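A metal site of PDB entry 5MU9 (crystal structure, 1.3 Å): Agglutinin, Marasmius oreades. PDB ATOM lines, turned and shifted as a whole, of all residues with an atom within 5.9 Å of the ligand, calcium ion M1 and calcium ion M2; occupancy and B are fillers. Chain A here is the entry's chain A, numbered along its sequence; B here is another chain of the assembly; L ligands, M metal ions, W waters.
The backbone NH (N) of Cys 215 is in hydrogen-bond range of an oxygen (O1) of the ligand, 2.8 Å away. The backbone carbonyl oxygen of Ala 256 lies within hydrogen-bond range of a nitrogen (N1) of the ligand. NE1 of Trp 208 is in hydrogen-bond range of O1 of the ligand (2.7 Å). C2 of the ligand is covalently linked to SG of Cys 215, at 1.9 Å.
O of His 257 is in hydrogen-bond range of N of Gly 248. N of Ala 258 sits at hydrogen-bond distance from SG of Cys 215 (3.6 Å). The backbone NH (N) of Tyr 289 is in hydrogen-bond range of the backbone carbonyl oxygen (O) of Leu 247 (2.8 Å). The side-chain amide oxygen (OE1) of Gln 211 sits at hydrogen-bond distance from the backbone NH (N) of Gly 184 of chain B (2.9 Å).
Residues that only touch the ligand: Tyr 289, His 257, Leu 247 and Ala 258. Hydrophobic or aromatic side chains within 4 Å of the ligand: Trp 208, Leu 247, Ala 256, His 257, Tyr 289 and Leu 182 of chain B. Within 4 Å of the ligand: Trp 208, Asp 214, Cys 215, Asp 216, Leu 247, Ala 256, His 257, Ala 258, Tyr 289 and Leu 182 of chain B. Along chain A the residues within 4 Å of the ligand span positions 208 to 289.
Four residues have an atom within 4 Å of calcium ion M1: Asp 214, Asp 216, Leu 182 of chain B and Asp 183 of chain B. The nearest printed residue that does not touch calcium ion M1 is Gln 211 (4.8 Å).
Of the 23 residues printed, 5 come within 4 Å of calcium ion M2. The nearest printed residue that does not touch calcium ion M2 is Ala 240 of chain B (4.4 Å).
O of Leu 182 of chain B is bound to calcium ion M1 (2.2 Å). OD1 of Asp 216 is bound to calcium ion M1 (2.3 Å). The side-chain carboxylate (OD1) of Asp 183 of chain B binds calcium ion M1. An oxygen (O4) of the ligand is bound to calcium ion M1. The side-chain carboxylate (OD2) of Asp 214 is bound to calcium ion M1. Water W2 binds calcium ion M1 (2.4 Å).
Calcium ion M2 is bound by O of Gln 211 (2.3 Å), OD2 of Asp 216 (2.4 Å), OD2 of Asp 217 (2.4 Å), OD1 of Asp 214 (2.4 Å), water W4 (2.4 Å), OD2 of Asp 183 of chain B (2.5 Å) and OD1 of Asp 183 of chain B (2.6 Å). Calcium ion M2 has seven donor atoms within binding distance.
Water W1 bridges an oxygen (O2) of the ligand and the side-chain amide nitrogen (NE2) of Gln 276. Water W3 lies within hydrogen-bond range of O5 of the ligand (2.8 Å) and N of Ala 256 (2.9 Å).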
ATOM      1  N   TRP A 208      -1.279  27.263 -15.718  1.00  0.00           N
ATOM      2  CA  TRP A 208      -0.729  25.933 -15.805  1.00  0.00           C
ATOM      3  C   TRP A 208       0.826  26.047 -15.682  1.00  0.00           C
ATOM      4  O   TRP A 208       1.437  26.826 -16.404  1.00  0.00           O
ATOM      5  CB  TRP A 208      -1.083  25.314 -17.149  1.00  0.00           C
ATOM      6  CG  TRP A 208      -0.617  23.861 -17.222  1.00  0.00           C
ATOM      7  CD1 TRP A 208      -1.305  22.726 -16.905  1.00  0.00           C
ATOM      8  CD2 TRP A 208       0.713  23.410 -17.570  1.00  0.00           C
ATOM      9  NE1 TRP A 208      -0.553  21.638 -17.044  1.00  0.00           N
ATOM     10  CE2 TRP A 208       0.684  22.000 -17.520  1.00  0.00           C
ATOM     11  CE3 TRP A 208       1.846  24.045 -18.047  1.00  0.00           C
ATOM     12  CZ2 TRP A 208       1.791  21.180 -17.811  1.00  0.00           C
ATOM     13  CZ3 TRP A 208       2.956  23.230 -18.399  1.00  0.00           C
ATOM     14  CH2 TRP A 208       2.918  21.826 -18.255  1.00  0.00           C
ATOM     15  N   GLN A 211       4.231  20.365 -13.233  1.00  0.00           N
ATOM     16  CA  GLN A 211       4.198  19.693 -11.943  1.00  0.00           C
ATOM     17  C   GLN A 211       3.681  20.535 -10.747  1.00  0.00           C
ATOM     18  O   GLN A 211       2.896  20.041  -9.930  1.00  0.00           O
ATOM     19  CB  GLN A 211       5.522  19.011 -11.552  1.00  0.00           C
ATOM     20  CG  GLN A 211       5.949  17.948 -12.552  1.00  0.00           C
ATOM     21  CD  GLN A 211       7.038  17.053 -11.949  1.00  0.00           C
ATOM     22  OE1 GLN A 211       6.971  16.593 -10.852  1.00  0.00           O
ATOM     23  NE2 GLN A 211       8.007  16.696 -12.830  1.00  0.00           N
ATOM     24  N   ILE A 212       4.157  21.785 -10.675  1.00  0.00           N
ATOM     25  CA  ILE A 212       3.844  22.598  -9.477  1.00  0.00           C
ATOM     26  C   ILE A 212       2.391  23.131  -9.480  1.00  0.00           C
ATOM     27  O   ILE A 212       1.879  23.475  -8.437  1.00  0.00           O
ATOM     28  CB  ILE A 212       4.917  23.702  -9.376  1.00  0.00           C
ATOM     29  CG1 ILE A 212       4.963  24.351  -7.980  1.00  0.00           C
ATOM     30  CG2 ILE A 212       4.811  24.738 -10.502  1.00  0.00           C
ATOM     31  CD1 ILE A 212       5.369  23.512  -6.783  1.00  0.00           C
ATOM     32  N   TYR A 213       1.841  23.273 -10.692  1.00  0.00           N
ATOM     33  CA  TYR A 213       0.385  23.630 -10.774  1.00  0.00           C
ATOM     34  C   TYR A 213      -0.169  23.157 -12.089  1.00  0.00           C
ATOM     35  O   TYR A 213      -0.469  23.938 -12.953  1.00  0.00           O
ATOM     36  CB  TYR A 213       0.089  25.096 -10.432  1.00  0.00           C
ATOM     37  CG  TYR A 213      -1.221  25.226  -9.670  1.00  0.00           C
ATOM     38  CD1 TYR A 213      -1.267  24.890  -8.282  1.00  0.00           C
ATOM     39  CD2 TYR A 213      -2.429  25.595 -10.269  1.00  0.00           C
ATOM     40  CE1 TYR A 213      -2.422  24.999  -7.527  1.00  0.00           C
ATOM     41  CE2 TYR A 213      -3.589  25.618  -9.537  1.00  0.00           C
ATOM     42  CZ  TYR A 213      -3.614  25.338  -8.204  1.00  0.00           C
ATOM     43  OH  TYR A 213      -4.821  25.391  -7.442  1.00  0.00           O
ATOM     44  N   ASP A 214      -0.313  21.836 -12.134  1.00  0.00           N
ATOM     45  CA  ASP A 214      -0.677  21.161 -13.421  1.00  0.00           C
ATOM     46  C   ASP A 214      -2.021  20.478 -13.211  1.00  0.00           C
ATOM     47  O   ASP A 214      -2.794  20.847 -12.288  1.00  0.00           O
ATOM     48  CB  ASP A 214       0.456  20.275 -13.936  1.00  0.00           C
ATOM     49  CG  ASP A 214       0.770  19.050 -13.072  1.00  0.00           C
ATOM     50  OD1 ASP A 214       0.463  19.149 -11.873  1.00  0.00           O
ATOM     51  OD2 ASP A 214       1.336  18.083 -13.606  1.00  0.00           O
ATOM     52  N   CYS A 215      -2.377  19.605 -14.128  1.00  0.00           N
ATOM     53  CA  CYS A 215      -3.767  19.082 -14.148  1.00  0.00           C
ATOM     54  C   CYS A 215      -4.259  18.557 -12.816  1.00  0.00           C
ATOM     55  O   CYS A 215      -5.379  18.857 -12.393  1.00  0.00           O
ATOM     56  CB  CYS A 215      -3.942  18.031 -15.298  1.00  0.00           C
ATOM     57  SG  CYS A 215      -2.742  16.674 -15.123  1.00  0.00           S
ATOM     58  N   ASP A 216      -3.439  17.795 -12.106  1.00  0.00           N
ATOM     59  CA  ASP A 216      -3.841  17.216 -10.865  1.00  0.00           C
ATOM     60  C   ASP A 216      -4.169  18.330  -9.800  1.00  0.00           C
ATOM     61  O   ASP A 216      -5.099  18.192  -8.992  1.00  0.00           O
ATOM     62  CB  ASP A 216      -2.872  16.204 -10.318  1.00  0.00           C
ATOM     63  CG  ASP A 216      -1.424  16.693 -10.433  1.00  0.00           C
ATOM     64  OD1 ASP A 216      -0.827  16.443 -11.497  1.00  0.00           O
ATOM     65  OD2 ASP A 216      -0.956  17.360  -9.453  1.00  0.00           O
ATOM     66  N   ASP A 217      -3.355  19.411  -9.832  1.00  0.00           N
ATOM     67  CA  ASP A 217      -3.599  20.476  -8.879  1.00  0.00           C
ATOM     68  C   ASP A 217      -4.951  21.218  -9.186  1.00  0.00           C
ATOM     69  O   ASP A 217      -5.715  21.524  -8.257  1.00  0.00           O
ATOM     70  CB  ASP A 217      -2.489  21.546  -8.960  1.00  0.00           C
ATOM     71  CG  ASP A 217      -1.122  20.889  -8.532  1.00  0.00           C
ATOM     72  OD1 ASP A 217      -0.987  20.663  -7.331  1.00  0.00           O
ATOM     73  OD2 ASP A 217      -0.368  20.507  -9.410  1.00  0.00           O
ATOM     74  N   MET A 246     -11.209  12.634 -11.586  1.00  0.00           N
ATOM     75  CA  MET A 246     -10.769  11.492 -12.393  1.00  0.00           C
ATOM     76  C   MET A 246      -9.308  11.647 -12.858  1.00  0.00           C
ATOM     77  O   MET A 246      -8.905  12.768 -13.226  1.00  0.00           O
ATOM     78  CB  MET A 246     -11.650  11.276 -13.620  1.00  0.00           C
ATOM     79  CG  MET A 246     -12.885  10.477 -13.335  1.00  0.00           C
ATOM     80  SD  MET A 246     -14.054  10.434 -14.658  1.00  0.00           S
ATOM     81  CE  MET A 246     -15.101   9.103 -14.023  1.00  0.00           C
ATOM     82  N   LEU A 247      -8.627  10.522 -12.948  1.00  0.00           N
ATOM     83  CA  LEU A 247      -7.415  10.347 -13.678  1.00  0.00           C
ATOM     84  C   LEU A 247      -7.701   9.534 -14.892  1.00  0.00           C
ATOM     85  O   LEU A 247      -8.369   8.451 -14.778  1.00  0.00           O
ATOM     86  CB  LEU A 247      -6.311   9.644 -12.809  1.00  0.00           C
ATOM     87  CG  LEU A 247      -6.191  10.258 -11.419  1.00  0.00           C
ATOM     88  CD1 LEU A 247      -5.052   9.515 -10.670  1.00  0.00           C
ATOM     89  CD2 LEU A 247      -5.928  11.752 -11.419  1.00  0.00           C
ATOM     90  N   GLY A 248      -7.260   9.923 -16.069  1.00  0.00           N
ATOM     91  CA  GLY A 248      -7.527   9.195 -17.331  1.00  0.00           C
ATOM     92  C   GLY A 248      -6.331   9.085 -18.236  1.00  0.00           C
ATOM     93  O   GLY A 248      -5.395   9.903 -18.103  1.00  0.00           O
ATOM     94  N   VAL A 249      -6.411   8.169 -19.204  1.00  0.00           N
ATOM     95  CA  VAL A 249      -5.401   7.924 -20.194  1.00  0.00           C
ATOM     96  C   VAL A 249      -6.022   7.965 -21.553  1.00  0.00           C
ATOM     97  O   VAL A 249      -7.193   7.603 -21.749  1.00  0.00           O
ATOM     98  CB  VAL A 249      -4.677   6.629 -19.888  1.00  0.00           C
ATOM     99  CG1 VAL A 249      -5.560   5.405 -19.961  1.00  0.00           C
ATOM    100  CG2 VAL A 249      -3.461   6.373 -20.787  1.00  0.00           C
ATOM    101  N   ALA A 255      -0.557   9.484 -23.133  1.00  0.00           N
ATOM    102  CA  ALA A 255      -0.794  10.777 -22.424  1.00  0.00           C
ATOM    103  C   ALA A 255      -1.848  10.502 -21.350  1.00  0.00           C
ATOM    104  O   ALA A 255      -2.778   9.738 -21.615  1.00  0.00           O
ATOM    105  CB  ALA A 255      -1.231  11.876 -23.431  1.00  0.00           C
ATOM    106  N   ALA A 256      -1.735  11.151 -20.183  1.00  0.00           N
ATOM    107  CA  ALA A 256      -2.722  11.054 -19.143  1.00  0.00           C
ATOM    108  C   ALA A 256      -3.018  12.438 -18.600  1.00  0.00           C
ATOM    109  O   ALA A 256      -2.246  13.386 -18.771  1.00  0.00           O
ATOM    110  CB  ALA A 256      -2.272  10.042 -18.110  1.00  0.00           C
ATOM    111  N   HIS A 257      -4.183  12.534 -17.998  1.00  0.00           N
ATOM    112  CA  HIS A 257      -4.767  13.810 -17.585  1.00  0.00           C
ATOM    113  C   HIS A 257      -5.608  13.654 -16.362  1.00  0.00           C
ATOM    114  O   HIS A 257      -6.223  12.599 -16.104  1.00  0.00           O
ATOM    115  CB  HIS A 257      -5.631  14.351 -18.775  1.00  0.00           C
ATOM    116  CG  HIS A 257      -6.049  15.747 -18.633  1.00  0.00           C
ATOM    117  ND1 HIS A 257      -5.205  16.737 -18.261  1.00  0.00           N
ATOM    118  CD2 HIS A 257      -7.278  16.314 -18.836  1.00  0.00           C
ATOM    119  CE1 HIS A 257      -5.867  17.897 -18.264  1.00  0.00           C
ATOM    120  NE2 HIS A 257      -7.148  17.661 -18.576  1.00  0.00           N
ATOM    121  N   ALA A 258      -5.719  14.715 -15.563  1.00  0.00           N
ATOM    122  CA  ALA A 258      -6.556  14.823 -14.364  1.00  0.00           C
ATOM    123  C   ALA A 258      -7.630  15.872 -14.595  1.00  0.00           C
ATOM    124  O   ALA A 258      -7.302  16.940 -15.098  1.00  0.00           O
ATOM    125  CB  ALA A 258      -5.767  15.096 -13.140  1.00  0.00           C
ATOM    126  N   GLN A 276      -9.175  23.572 -15.885  1.00  0.00           N
ATOM    127  CA  GLN A 276      -8.304  24.605 -16.446  1.00  0.00           C
ATOM    128  C   GLN A 276      -9.071  25.632 -17.328  1.00  0.00           C
ATOM    129  O   GLN A 276      -8.567  26.731 -17.544  1.00  0.00           O
ATOM    130  CB  GLN A 276      -7.215  23.938 -17.301  1.00  0.00           C
ATOM    131  CG  GLN A 276      -6.206  23.252 -16.521  1.00  0.00           C
ATOM    132  CD  GLN A 276      -5.124  22.704 -17.398  1.00  0.00           C
ATOM    133  OE1 GLN A 276      -4.452  23.414 -18.117  1.00  0.00           O
ATOM    134  NE2 GLN A 276      -4.889  21.407 -17.244  1.00  0.00           N
ATOM    135  N   TYR A 289      -9.075   5.865 -15.465  1.00  0.00           N
ATOM    136  CA  TYR A 289      -8.594   4.754 -14.726  1.00  0.00           C
ATOM    137  C   TYR A 289      -8.703   4.814 -13.245  1.00  0.00           C
ATOM    138  O   TYR A 289      -8.547   3.824 -12.571  1.00  0.00           O
ATOM    139  CB  TYR A 289      -7.115   4.395 -15.156  1.00  0.00           C
ATOM    140  CG  TYR A 289      -6.071   5.445 -14.812  1.00  0.00           C
ATOM    141  CD1 TYR A 289      -5.431   5.433 -13.600  1.00  0.00           C
ATOM    142  CD2 TYR A 289      -5.733   6.418 -15.707  1.00  0.00           C
ATOM    143  CE1 TYR A 289      -4.466   6.356 -13.263  1.00  0.00           C
ATOM    144  CE2 TYR A 289      -4.737   7.325 -15.422  1.00  0.00           C
ATOM    145  CZ  TYR A 289      -4.125   7.322 -14.170  1.00  0.00           C
ATOM    146  OH  TYR A 289      -3.165   8.265 -13.914  1.00  0.00           O
ATOM    147  N   ILE B 181      -0.032   8.003  -8.500  1.00  0.00           N
ATOM    148  CA  ILE B 181       1.061   8.938  -8.545  1.00  0.00           C
ATOM    149  C   ILE B 181       0.716  10.060  -9.496  1.00  0.00           C
ATOM    150  O   ILE B 181       0.221   9.872 -10.617  1.00  0.00           O
ATOM    151  CB  ILE B 181       2.369   8.251  -9.024  1.00  0.00           C
ATOM    152  CG1 ILE B 181       2.807   7.255  -7.978  1.00  0.00           C
ATOM    153  CG2 ILE B 181       3.413   9.271  -9.331  1.00  0.00           C
ATOM    154  CD1 ILE B 181       3.973   6.432  -8.406  1.00  0.00           C
ATOM    155  N   LEU B 182       0.832  11.298  -9.015  1.00  0.00           N
ATOM    156  CA  LEU B 182       0.401  12.494  -9.753  1.00  0.00           C
ATOM    157  C   LEU B 182       1.489  13.288 -10.417  1.00  0.00           C
ATOM    158  O   LEU B 182       1.231  14.088 -11.384  1.00  0.00           O
ATOM    159  CB  LEU B 182      -0.445  13.401  -8.848  1.00  0.00           C
ATOM    160  CG  LEU B 182      -1.616  12.706  -8.184  1.00  0.00           C
ATOM    161  CD1 LEU B 182      -2.275  13.628  -7.090  1.00  0.00           C
ATOM    162  CD2 LEU B 182      -2.696  12.273  -9.172  1.00  0.00           C
ATOM    163  N   ASP B 183       2.714  13.280  -9.813  1.00  0.00           N
ATOM    164  CA  ASP B 183       3.836  14.120 -10.248  1.00  0.00           C
ATOM    165  C   ASP B 183       5.083  13.250 -10.271  1.00  0.00           C
ATOM    166  O   ASP B 183       5.027  12.061  -9.999  1.00  0.00           O
ATOM    167  CB  ASP B 183       3.989  15.383  -9.447  1.00  0.00           C
ATOM    168  CG  ASP B 183       2.690  16.329  -9.572  1.00  0.00           C
ATOM    169  OD1 ASP B 183       2.495  16.758 -10.731  1.00  0.00           O
ATOM    170  OD2 ASP B 183       2.124  16.655  -8.513  1.00  0.00           O
ATOM    171  N   GLY B 184       6.211  13.840 -10.571  1.00  0.00           N
ATOM    172  CA  GLY B 184       7.502  13.129 -10.764  1.00  0.00           C
ATOM    173  C   GLY B 184       8.583  13.383  -9.718  1.00  0.00           C
ATOM    174  O   GLY B 184       9.383  12.474  -9.452  1.00  0.00           O
ATOM    175  N   ALA B 240       6.883  19.252  -7.680  1.00  0.00           N
ATOM    176  CA  ALA B 240       5.713  19.436  -6.855  1.00  0.00           C
ATOM    177  C   ALA B 240       6.115  19.392  -5.372  1.00  0.00           C
ATOM    178  O   ALA B 240       7.261  19.177  -5.029  1.00  0.00           O
ATOM    179  CB  ALA B 240       4.708  18.291  -7.184  1.00  0.00           C
HETATM  180  C1  LIG L   1      -1.654  18.068 -17.410  1.00  0.00           C
HETATM  181  O1  LIG L   1      -1.305  19.044 -16.656  1.00  0.00           O
HETATM  182  O2  LIG L   1      -1.982  18.098 -18.702  1.00  0.00           O
HETATM  183  C2  LIG L   1      -1.670  16.661 -16.724  1.00  0.00           C
HETATM  184  C3  LIG L   1      -0.231  16.408 -16.364  1.00  0.00           C
HETATM  185  O3  LIG L   1       0.423  16.032 -17.651  1.00  0.00           O
HETATM  186  C4  LIG L   1      -0.154  15.125 -15.489  1.00  0.00           C
HETATM  187  O4  LIG L   1       0.078  15.048 -14.324  1.00  0.00           O
HETATM  188  N1  LIG L   1      -0.203  13.959 -16.201  1.00  0.00           N
HETATM  189  C5  LIG L   1       0.071  12.730 -15.494  1.00  0.00           C
HETATM  190  C6  LIG L   1      -1.265  11.941 -15.268  1.00  0.00           C
HETATM  191  C7  LIG L   1      -2.354  12.542 -14.357  1.00  0.00           C
HETATM  192  C8  LIG L   1      -1.959  12.661 -12.948  1.00  0.00           C
HETATM  193  C9  LIG L   1      -3.556  11.631 -14.432  1.00  0.00           C
HETATM  194  C10 LIG L   1       0.908  11.747 -16.305  1.00  0.00           C
HETATM  195  O5  LIG L   1       0.888  11.868 -17.510  1.00  0.00           O
HETATM  196  N2  LIG L   1       1.574  10.749 -15.678  1.00  0.00           N
HETATM  197  C11 LIG L   1       2.428   9.767 -16.369  1.00  0.00           C
HETATM  198  C12 LIG L   1       1.833   8.374 -16.398  1.00  0.00           C
HETATM  199  C13 LIG L   1       1.065   7.993 -15.125  1.00  0.00           C
HETATM  200  C14 LIG L   1      -0.425   8.000 -15.425  1.00  0.00           C
HETATM  201  N3  LIG L   1      -0.920   6.924 -16.308  1.00  0.00           N
HETATM  202  C15 LIG L   1      -1.243   5.696 -15.826  1.00  0.00           C
HETATM  203  N4  LIG L   1      -2.103   4.922 -16.481  1.00  0.00           N
HETATM  204  N5  LIG L   1      -0.831   5.259 -14.626  1.00  0.00           N
HETATM  205 CA    CA M   1       1.214  16.012 -12.528  1.00  0.00          CA
HETATM  206 CA    CA M   2       1.070  18.613  -9.626  1.00  0.00          CA
HETATM  207  O   HOH W   1      -3.118  20.256 -19.324  1.00  0.00           O
HETATM  208  O   HOH W   2       3.188  15.369 -13.673  1.00  0.00           O
HETATM  209  O   HOH W   3       0.750  12.692 -20.165  1.00  0.00           O
HETATM  210  O   HOH W   4       1.075  19.043  -7.221  1.00  0.00           O
